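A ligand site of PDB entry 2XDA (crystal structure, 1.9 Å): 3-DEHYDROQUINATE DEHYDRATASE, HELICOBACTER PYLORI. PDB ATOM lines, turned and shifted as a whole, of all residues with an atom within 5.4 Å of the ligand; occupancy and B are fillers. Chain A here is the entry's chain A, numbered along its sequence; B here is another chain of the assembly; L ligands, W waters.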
ATOM      1  N   PRO A   9       6.642  16.656 -11.904  1.00  0.00           N
ATOM      2  CA  PRO A   9       8.007  16.403 -11.470  1.00  0.00           C
ATOM      3  C   PRO A   9       8.202  14.964 -11.044  1.00  0.00           C
ATOM      4  O   PRO A   9       7.360  14.375 -10.391  1.00  0.00           O
ATOM      5  CB  PRO A   9       8.219  17.385 -10.316  1.00  0.00           C
ATOM      6  CG  PRO A   9       6.871  17.765  -9.859  1.00  0.00           C
ATOM      7  CD  PRO A   9       6.010  17.716 -11.109  1.00  0.00           C
ATOM      8  N   ASN A  10       9.334  14.430 -11.475  1.00  0.00           N
ATOM      9  CA  ASN A  10       9.804  13.099 -11.159  1.00  0.00           C
ATOM     10  C   ASN A  10       9.117  11.956 -11.894  1.00  0.00           C
ATOM     11  O   ASN A  10       9.647  10.860 -11.855  1.00  0.00           O
ATOM     12  CB  ASN A  10       9.767  12.824  -9.642  1.00  0.00           C
ATOM     13  CG  ASN A  10      10.628  13.792  -8.870  1.00  0.00           C
ATOM     14  OD1 ASN A  10      11.831  13.868  -9.114  1.00  0.00           O
ATOM     15  ND2 ASN A  10       9.993  14.624  -8.002  1.00  0.00           N
ATOM     16  N   LEU A  11       8.003  12.215 -12.597  1.00  0.00           N
ATOM     17  CA  LEU A  11       7.270  11.125 -13.291  1.00  0.00           C
ATOM     18  C   LEU A  11       8.137  10.426 -14.359  1.00  0.00           C
ATOM     19  O   LEU A  11       7.922   9.236 -14.659  1.00  0.00           O
ATOM     20  CB  LEU A  11       6.017  11.622 -13.949  1.00  0.00           C
ATOM     21  CG  LEU A  11       4.703  11.592 -13.166  1.00  0.00           C
ATOM     22  CD1 LEU A  11       4.299  10.086 -12.918  1.00  0.00           C
ATOM     23  CD2 LEU A  11       4.761  12.450 -11.901  1.00  0.00           C
ATOM     24  N   MET A  13      11.006   9.382 -14.066  1.00  0.00           N
ATOM     25  CA  MET A  13      11.779   8.334 -13.406  1.00  0.00           C
ATOM     26  C   MET A  13      10.989   7.065 -13.114  1.00  0.00           C
ATOM     27  O   MET A  13      11.535   6.125 -12.558  1.00  0.00           O
ATOM     28  CB  MET A  13      12.433   8.852 -12.129  1.00  0.00           C
ATOM     29  CG  MET A  13      13.258  10.109 -12.326  1.00  0.00           C
ATOM     30  SD  MET A  13      14.491  10.051 -13.652  1.00  0.00           S
ATOM     31  CE  MET A  13      15.969   9.555 -12.777  1.00  0.00           C
ATOM     32  N   LEU A  14       9.713   7.023 -13.482  1.00  0.00           N
ATOM     33  CA  LEU A  14       8.840   5.908 -13.217  1.00  0.00           C
ATOM     34  C   LEU A  14       9.419   4.649 -13.845  1.00  0.00           C
ATOM     35  O   LEU A  14       9.942   4.683 -14.967  1.00  0.00           O
ATOM     36  CB  LEU A  14       7.448   6.200 -13.778  1.00  0.00           C
ATOM     37  CG  LEU A  14       6.311   5.290 -13.398  1.00  0.00           C
ATOM     38  CD1 LEU A  14       6.158   5.183 -11.869  1.00  0.00           C
ATOM     39  CD2 LEU A  14       5.057   5.815 -14.086  1.00  0.00           C
ATOM     40  N   GLY A  15       9.368   3.553 -13.092  1.00  0.00           N
ATOM     41  CA  GLY A  15       9.848   2.285 -13.576  1.00  0.00           C
ATOM     42  C   GLY A  15      11.330   2.110 -13.360  1.00  0.00           C
ATOM     43  O   GLY A  15      11.807   0.980 -13.358  1.00  0.00           O
ATOM     44  N   ARG A  17      13.051   3.990 -10.694  1.00  0.00           N
ATOM     45  CA  ARG A  17      13.323   4.227  -9.287  1.00  0.00           C
ATOM     46  C   ARG A  17      12.133   3.846  -8.412  1.00  0.00           C
ATOM     47  O   ARG A  17      10.997   3.922  -8.847  1.00  0.00           O
ATOM     48  CB  ARG A  17      13.683   5.706  -9.066  1.00  0.00           C
ATOM     49  CG  ARG A  17      15.006   6.156  -9.718  1.00  0.00           C
ATOM     50  CD  ARG A  17      16.161   5.332  -9.200  1.00  0.00           C
ATOM     51  NE  ARG A  17      17.472   5.969  -9.346  1.00  0.00           N
ATOM     52  CZ  ARG A  17      18.621   5.425  -8.932  1.00  0.00           C
ATOM     53  NH1 ARG A  17      18.641   4.213  -8.370  1.00  0.00           N
ATOM     54  NH2 ARG A  17      19.778   6.081  -9.095  1.00  0.00           N
ATOM     55  N   ASP A  18      12.442   3.420  -7.177  1.00  0.00           N
ATOM     56  CA  ASP A  18      11.456   3.000  -6.165  1.00  0.00           C
ATOM     57  C   ASP A  18      10.314   2.136  -6.704  1.00  0.00           C
ATOM     58  O   ASP A  18       9.133   2.467  -6.532  1.00  0.00           O
ATOM     59  CB  ASP A  18      10.900   4.210  -5.427  1.00  0.00           C
ATOM     60  CG  ASP A  18      10.234   3.818  -4.095  1.00  0.00           C
ATOM     61  OD1 ASP A  18      10.103   2.600  -3.791  1.00  0.00           O
ATOM     62  OD2 ASP A  18       9.840   4.760  -3.354  1.00  0.00           O
ATOM     63  N   TYR A  22       6.150   2.563  -6.674  1.00  0.00           N
ATOM     64  CA  TYR A  22       5.594   3.127  -7.915  1.00  0.00           C
ATOM     65  C   TYR A  22       5.555   2.150  -9.086  1.00  0.00           C
ATOM     66  O   TYR A  22       5.055   2.486 -10.160  1.00  0.00           O
ATOM     67  CB  TYR A  22       6.372   4.367  -8.307  1.00  0.00           C
ATOM     68  CG  TYR A  22       6.206   5.540  -7.363  1.00  0.00           C
ATOM     69  CD1 TYR A  22       7.253   5.938  -6.536  1.00  0.00           C
ATOM     70  CD2 TYR A  22       5.024   6.256  -7.315  1.00  0.00           C
ATOM     71  CE1 TYR A  22       7.100   7.022  -5.672  1.00  0.00           C
ATOM     72  CE2 TYR A  22       4.868   7.326  -6.454  1.00  0.00           C
ATOM     73  CZ  TYR A  22       5.891   7.717  -5.640  1.00  0.00           C
ATOM     74  OH  TYR A  22       5.756   8.801  -4.793  1.00  0.00           O
ATOM     75  N   ASN A  76      -1.089  14.522 -13.838  1.00  0.00           N
ATOM     76  CA  ASN A  76      -0.527  14.058 -12.590  1.00  0.00           C
ATOM     77  C   ASN A  76       0.511  15.102 -12.221  1.00  0.00           C
ATOM     78  O   ASN A  76       1.617  15.022 -12.692  1.00  0.00           O
ATOM     79  CB  ASN A  76       0.130  12.680 -12.736  1.00  0.00           C
ATOM     80  CG  ASN A  76       0.682  12.155 -11.434  1.00  0.00           C
ATOM     81  OD1 ASN A  76       0.909  12.905 -10.452  1.00  0.00           O
ATOM     82  ND2 ASN A  76       0.882  10.859 -11.393  1.00  0.00           N
ATOM     83  N   PRO A  77       0.168  16.036 -11.306  1.00  0.00           N
ATOM     84  CA  PRO A  77       1.135  17.108 -11.009  1.00  0.00           C
ATOM     85  C   PRO A  77       2.281  16.676 -10.093  1.00  0.00           C
ATOM     86  O   PRO A  77       3.074  17.512  -9.694  1.00  0.00           O
ATOM     87  CB  PRO A  77       0.290  18.180 -10.320  1.00  0.00           C
ATOM     88  CG  PRO A  77      -1.118  17.783 -10.472  1.00  0.00           C
ATOM     89  CD  PRO A  77      -1.142  16.289 -10.694  1.00  0.00           C
ATOM     90  N   GLY A  78       2.328  15.410  -9.724  1.00  0.00           N
ATOM     91  CA  GLY A  78       3.344  14.937  -8.806  1.00  0.00           C
ATOM     92  C   GLY A  78       3.268  15.739  -7.491  1.00  0.00           C
ATOM     93  O   GLY A  78       2.190  16.123  -7.028  1.00  0.00           O
ATOM     94  N   ALA A  79       4.426  16.063  -6.953  1.00  0.00           N
ATOM     95  CA  ALA A  79       4.516  16.740  -5.690  1.00  0.00           C
ATOM     96  C   ALA A  79       3.926  18.164  -5.726  1.00  0.00           C
ATOM     97  O   ALA A  79       3.510  18.708  -4.699  1.00  0.00           O
ATOM     98  CB  ALA A  79       5.995  16.783  -5.234  1.00  0.00           C
ATOM     99  N   SER A  81       1.088  18.874  -6.694  1.00  0.00           N
ATOM    100  CA  SER A  81      -0.292  18.740  -6.241  1.00  0.00           C
ATOM    101  C   SER A  81      -0.453  19.400  -4.872  1.00  0.00           C
ATOM    102  O   SER A  81      -1.461  20.052  -4.600  1.00  0.00           O
ATOM    103  CB  SER A  81      -0.702  17.263  -6.168  1.00  0.00           C
ATOM    104  OG  SER A  81      -0.417  16.625  -7.439  1.00  0.00           O
ATOM    105  N   HIS A  82       0.525  19.195  -4.005  1.00  0.00           N
ATOM    106  CA  HIS A  82       0.373  19.554  -2.604  1.00  0.00           C
ATOM    107  C   HIS A  82       0.808  20.984  -2.325  1.00  0.00           C
ATOM    108  O   HIS A  82       0.499  21.505  -1.253  1.00  0.00           O
ATOM    109  CB  HIS A  82       1.201  18.606  -1.732  1.00  0.00           C
ATOM    110  CG  HIS A  82       1.113  17.190  -2.205  1.00  0.00           C
ATOM    111  ND1 HIS A  82      -0.073  16.488  -2.224  1.00  0.00           N
ATOM    112  CD2 HIS A  82       2.063  16.360  -2.700  1.00  0.00           C
ATOM    113  CE1 HIS A  82       0.154  15.282  -2.738  1.00  0.00           C
ATOM    114  NE2 HIS A  82       1.446  15.178  -3.013  1.00  0.00           N
ATOM    115  N   VAL A 101      -4.767  12.584 -11.797  1.00  0.00           N
ATOM    116  CA  VAL A 101      -4.432  11.229 -11.526  1.00  0.00           C
ATOM    117  C   VAL A 101      -3.213  11.145 -10.622  1.00  0.00           C
ATOM    118  O   VAL A 101      -2.230  11.860 -10.833  1.00  0.00           O
ATOM    119  CB  VAL A 101      -4.078  10.498 -12.843  1.00  0.00           C
ATOM    120  CG1 VAL A 101      -3.517   9.098 -12.534  1.00  0.00           C
ATOM    121  CG2 VAL A 101      -5.279  10.433 -13.791  1.00  0.00           C
ATOM    122  N   HIS A 102      -3.272  10.286  -9.616  1.00  0.00           N
ATOM    123  CA  HIS A 102      -2.100   9.873  -8.853  1.00  0.00           C
ATOM    124  C   HIS A 102      -1.970   8.383  -8.913  1.00  0.00           C
ATOM    125  O   HIS A 102      -2.966   7.658  -8.826  1.00  0.00           O
ATOM    126  CB  HIS A 102      -2.222  10.269  -7.376  1.00  0.00           C
ATOM    127  CG  HIS A 102      -2.366  11.730  -7.196  1.00  0.00           C
ATOM    128  ND1 HIS A 102      -1.304  12.590  -7.327  1.00  0.00           N
ATOM    129  CD2 HIS A 102      -3.466  12.492  -7.017  1.00  0.00           C
ATOM    130  CE1 HIS A 102      -1.746  13.830  -7.178  1.00  0.00           C
ATOM    131  NE2 HIS A 102      -3.046  13.792  -6.992  1.00  0.00           N
ATOM    132  N   LEU A 103      -0.732   7.941  -9.068  1.00  0.00           N
ATOM    133  CA  LEU A 103      -0.413   6.508  -9.046  1.00  0.00           C
ATOM    134  C   LEU A 103      -0.760   5.909  -7.698  1.00  0.00           C
ATOM    135  O   LEU A 103      -1.374   4.817  -7.618  1.00  0.00           O
ATOM    136  CB  LEU A 103       1.080   6.281  -9.349  1.00  0.00           C
ATOM    137  CG  LEU A 103       1.557   6.708 -10.734  1.00  0.00           C
ATOM    138  CD1 LEU A 103       3.081   6.791 -10.744  1.00  0.00           C
ATOM    139  CD2 LEU A 103       1.080   5.717 -11.808  1.00  0.00           C
ATOM    140  N   THR A 104      -0.355   6.619  -6.656  1.00  0.00           N
ATOM    141  CA  THR A 104      -0.576   6.197  -5.285  1.00  0.00           C
ATOM    142  C   THR A 104      -1.801   6.852  -4.673  1.00  0.00           C
ATOM    143  O   THR A 104      -2.347   7.822  -5.200  1.00  0.00           O
ATOM    144  CB  THR A 104       0.645   6.452  -4.391  1.00  0.00           C
ATOM    145  OG1 THR A 104       0.915   7.875  -4.280  1.00  0.00           O
ATOM    146  CG2 THR A 104       1.884   5.722  -4.971  1.00  0.00           C
ATOM    147  N   ILE A 106      -2.898   9.085  -2.202  1.00  0.00           N
ATOM    148  CA  ILE A 106      -2.373  10.183  -1.418  1.00  0.00           C
ATOM    149  C   ILE A 106      -3.112  10.473  -0.125  1.00  0.00           C
ATOM    150  O   ILE A 106      -2.693  11.361   0.604  1.00  0.00           O
ATOM    151  CB  ILE A 106      -2.186  11.502  -2.242  1.00  0.00           C
ATOM    152  CG1 ILE A 106      -3.525  12.026  -2.772  1.00  0.00           C
ATOM    153  CG2 ILE A 106      -1.156  11.232  -3.301  1.00  0.00           C
ATOM    154  CD1 ILE A 106      -3.453  13.509  -3.241  1.00  0.00           C
ATOM    155  N   ARG A 109      -0.668   8.102   2.702  1.00  0.00           N
ATOM    156  CA  ARG A 109       0.760   8.304   2.851  1.00  0.00           C
ATOM    157  C   ARG A 109       1.091   9.355   3.915  1.00  0.00           C
ATOM    158  O   ARG A 109       0.369   9.494   4.923  1.00  0.00           O
ATOM    159  CB  ARG A 109       1.361   8.621   1.452  1.00  0.00           C
ATOM    160  CG  ARG A 109       1.144   7.487   0.469  1.00  0.00           C
ATOM    161  CD  ARG A 109       1.749   7.797  -0.902  1.00  0.00           C
ATOM    162  NE  ARG A 109       3.198   7.960  -0.831  1.00  0.00           N
ATOM    163  CZ  ARG A 109       3.962   8.342  -1.842  1.00  0.00           C
ATOM    164  NH1 ARG A 109       3.439   8.643  -3.009  1.00  0.00           N
ATOM    165  NH2 ARG A 109       5.277   8.451  -1.662  1.00  0.00           N
ATOM    166  N   ARG A 113       1.114  14.889   2.015  1.00  0.00           N
ATOM    167  CA  ARG A 113       0.546  14.567   0.697  1.00  0.00           C
ATOM    168  C   ARG A 113      -0.960  14.622   0.626  1.00  0.00           C
ATOM    169  O   ARG A 113      -1.534  14.503  -0.454  1.00  0.00           O
ATOM    170  CB  ARG A 113       1.017  13.202   0.192  1.00  0.00           C
ATOM    171  CG  ARG A 113       2.501  13.103   0.066  1.00  0.00           C
ATOM    172  CD  ARG A 113       2.927  11.827  -0.654  1.00  0.00           C
ATOM    173  NE  ARG A 113       4.340  11.585  -0.363  1.00  0.00           N
ATOM    174  CZ  ARG A 113       5.369  12.051  -1.063  1.00  0.00           C
ATOM    175  NH1 ARG A 113       5.192  12.771  -2.170  1.00  0.00           N
ATOM    176  NH2 ARG A 113       6.585  11.785  -0.640  1.00  0.00           N
ATOM    177  N   ILE B  85       8.545  19.706  -1.811  1.00  0.00           N
ATOM    178  CA  ILE B  85       8.303  18.284  -1.772  1.00  0.00           C
ATOM    179  C   ILE B  85       8.858  17.608  -3.047  1.00  0.00           C
ATOM    180  O   ILE B  85       9.370  16.494  -2.980  1.00  0.00           O
ATOM    181  CB  ILE B  85       6.809  17.943  -1.533  1.00  0.00           C
ATOM    182  CG1 ILE B  85       6.346  18.526  -0.175  1.00  0.00           C
ATOM    183  CG2 ILE B  85       6.572  16.448  -1.570  1.00  0.00           C
ATOM    184  CD1 ILE B  85       4.815  18.613  -0.016  1.00  0.00           C
ATOM    185  N   ASP B  89      11.399  14.552  -3.057  1.00  0.00           N
ATOM    186  CA  ASP B  89      11.149  13.300  -3.784  1.00  0.00           C
ATOM    187  C   ASP B  89      12.324  12.954  -4.713  1.00  0.00           C
ATOM    188  O   ASP B  89      12.725  11.777  -4.806  1.00  0.00           O
ATOM    189  CB  ASP B  89       9.806  13.331  -4.521  1.00  0.00           C
ATOM    190  CG  ASP B  89       8.589  13.089  -3.581  1.00  0.00           C
ATOM    191  OD1 ASP B  89       8.760  12.710  -2.411  1.00  0.00           O
ATOM    192  OD2 ASP B  89       7.457  13.319  -4.018  1.00  0.00           O
ATOM    193  N   LEU B  93      14.575   9.636  -4.559  1.00  0.00           N
ATOM    194  CA  LEU B  93      14.679   8.768  -5.717  1.00  0.00           C
ATOM    195  C   LEU B  93      16.090   8.664  -6.296  1.00  0.00           C
ATOM    196  O   LEU B  93      16.356   7.767  -7.103  1.00  0.00           O
ATOM    197  CB  LEU B  93      13.721   9.259  -6.786  1.00  0.00           C
ATOM    198  CG  LEU B  93      12.249   9.173  -6.374  1.00  0.00           C
ATOM    199  CD1 LEU B  93      11.456  10.091  -7.310  1.00  0.00           C
ATOM    200  CD2 LEU B  93      11.768   7.731  -6.437  1.00  0.00           C
HETATM  201  C1  LIG L   1       8.368   8.007  -9.958  1.00  0.00           C
HETATM  202  C2  LIG L   1       7.550   8.860  -8.979  1.00  0.00           C
HETATM  203  C3  LIG L   1       6.627   9.891  -9.657  1.00  0.00           C
HETATM  204  C4  LIG L   1       5.700  10.467  -8.579  1.00  0.00           C
HETATM  205  C5  LIG L   1       4.357  10.408  -8.502  1.00  0.00           C
HETATM  206  S1  LIG L   1       6.274  11.307  -7.290  1.00  0.00           S
HETATM  207  C6  LIG L   1       4.775  11.594  -6.620  1.00  0.00           C
HETATM  208  C7  LIG L   1       3.795  11.016  -7.425  1.00  0.00           C
HETATM  209  C8  LIG L   1       2.294  11.103  -7.043  1.00  0.00           C
HETATM  210  C9  LIG L   1       1.595   9.817  -7.486  1.00  0.00           C
HETATM  211  O1  LIG L   1       1.276   9.801  -8.667  1.00  0.00           O
HETATM  212  O2  LIG L   1       1.369   8.895  -6.661  1.00  0.00           O
HETATM  213  O3  LIG L   1       1.627  12.180  -7.762  1.00  0.00           O
HETATM  214  C10 LIG L   1       2.120  11.401  -5.536  1.00  0.00           C
HETATM  215  C11 LIG L   1       3.001  12.604  -5.152  1.00  0.00           C
HETATM  216  O4  LIG L   1       2.818  12.903  -3.754  1.00  0.00           O
HETATM  217  C12 LIG L   1       4.483  12.287  -5.321  1.00  0.00           C
HETATM  218  O5  LIG L   1       5.359  13.424  -5.186  1.00  0.00           O
HETATM  219  C13 LIG L   1       9.038   6.769  -9.356  1.00  0.00           C
HETATM  220  C14 LIG L   1       9.875   7.972  -9.729  1.00  0.00           C
HETATM  221  O   HOH W   1       6.956  14.695  -7.674  1.00  0.00           O
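The side-chain carboxylate (OD2) of Asp 89 of chain B sits at hydrogen-bond distance from an oxygen (O5) of the ligand, at 2.4 Å. N of Thr 104 sits at hydrogen-bond distance from O2 of the ligand (2.9 Å). OG1 of Thr 104 is in hydrogen-bond range of O2 of the ligand (2.6 Å). NE2 of His 82 is in hydrogen-bond range of O4 of the ligand (2.8 Å). O1 of the ligand sits at hydrogen-bond distance from N of Leu 103 (2.8 Å). NH1 of Arg 113 is in hydrogen-bond range of O4 of the ligand. O3 of the ligand lies within hydrogen-bond range of OD1 of Asn 76, 2.9 Å away. An oxygen (O3) of the ligand sits at hydrogen-bond distance from a ring nitrogen (ND1) of His 102. N of Ala 79 lies within hydrogen-bond range of O5 of the ligand, at 3.3 Å. The side-chain hydroxyl of Tyr 22 sits close to a sulfur (S1) of the ligand.
Residues that only touch the ligand: Asn 10 (3.6 Å), Leu 11 (3.9 Å), Met 13 (3.6 Å), Leu 14 (3.9 Å), Arg 17 (3.5 Å), Gly 78 (3.4 Å), Ile 106 (3.97 Å), Arg 109 (3.97 Å) and Leu 93 of chain B (3.6 Å). Of the 25 residues printed, 18 come within 4 Å of the ligand. The nearest printed residue that does not touch the ligand is Pro 9 (4.5 Å).
The side-chain carboxylate of Asp 89 of chain B is in salt-bridge range of the guanidinium group of Arg 113 (3.0 Å). OG1 of Thr 104 is in hydrogen-bond range of NH1 of Arg 109. A ring nitrogen (ND1) of His 82 lies close to the backbone carbonyl oxygen (O) of Arg 113, 3.0 Å away. The backbone NH of Gly 78 sits at hydrogen-bond distance from the side-chain amide oxygen of Asn 76 (3.0 Å). The side-chain amide nitrogen of Asn 76 lies close to the backbone carbonyl oxygen of Val 101 (3.3 Å). The side-chain hydroxyl (OG) of Ser 81 sits at hydrogen-bond distance from the backbone carbonyl oxygen (O) of Gly 78 (2.7 Å). The side-chain hydroxyl (OH) of Tyr 22 lies within hydrogen-bond range of the guanidinium group (NH1) of Arg 109 (2.9 Å). The guanidinium group of Arg 17 lies within hydrogen-bond range of the backbone carbonyl oxygen of Leu 93 of chain B (3.1 Å).
Water W1 lies within hydrogen-bond range of O of Pro 9, N of Ala 79, ND2 of Asn 10 and O5 of the ligand.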
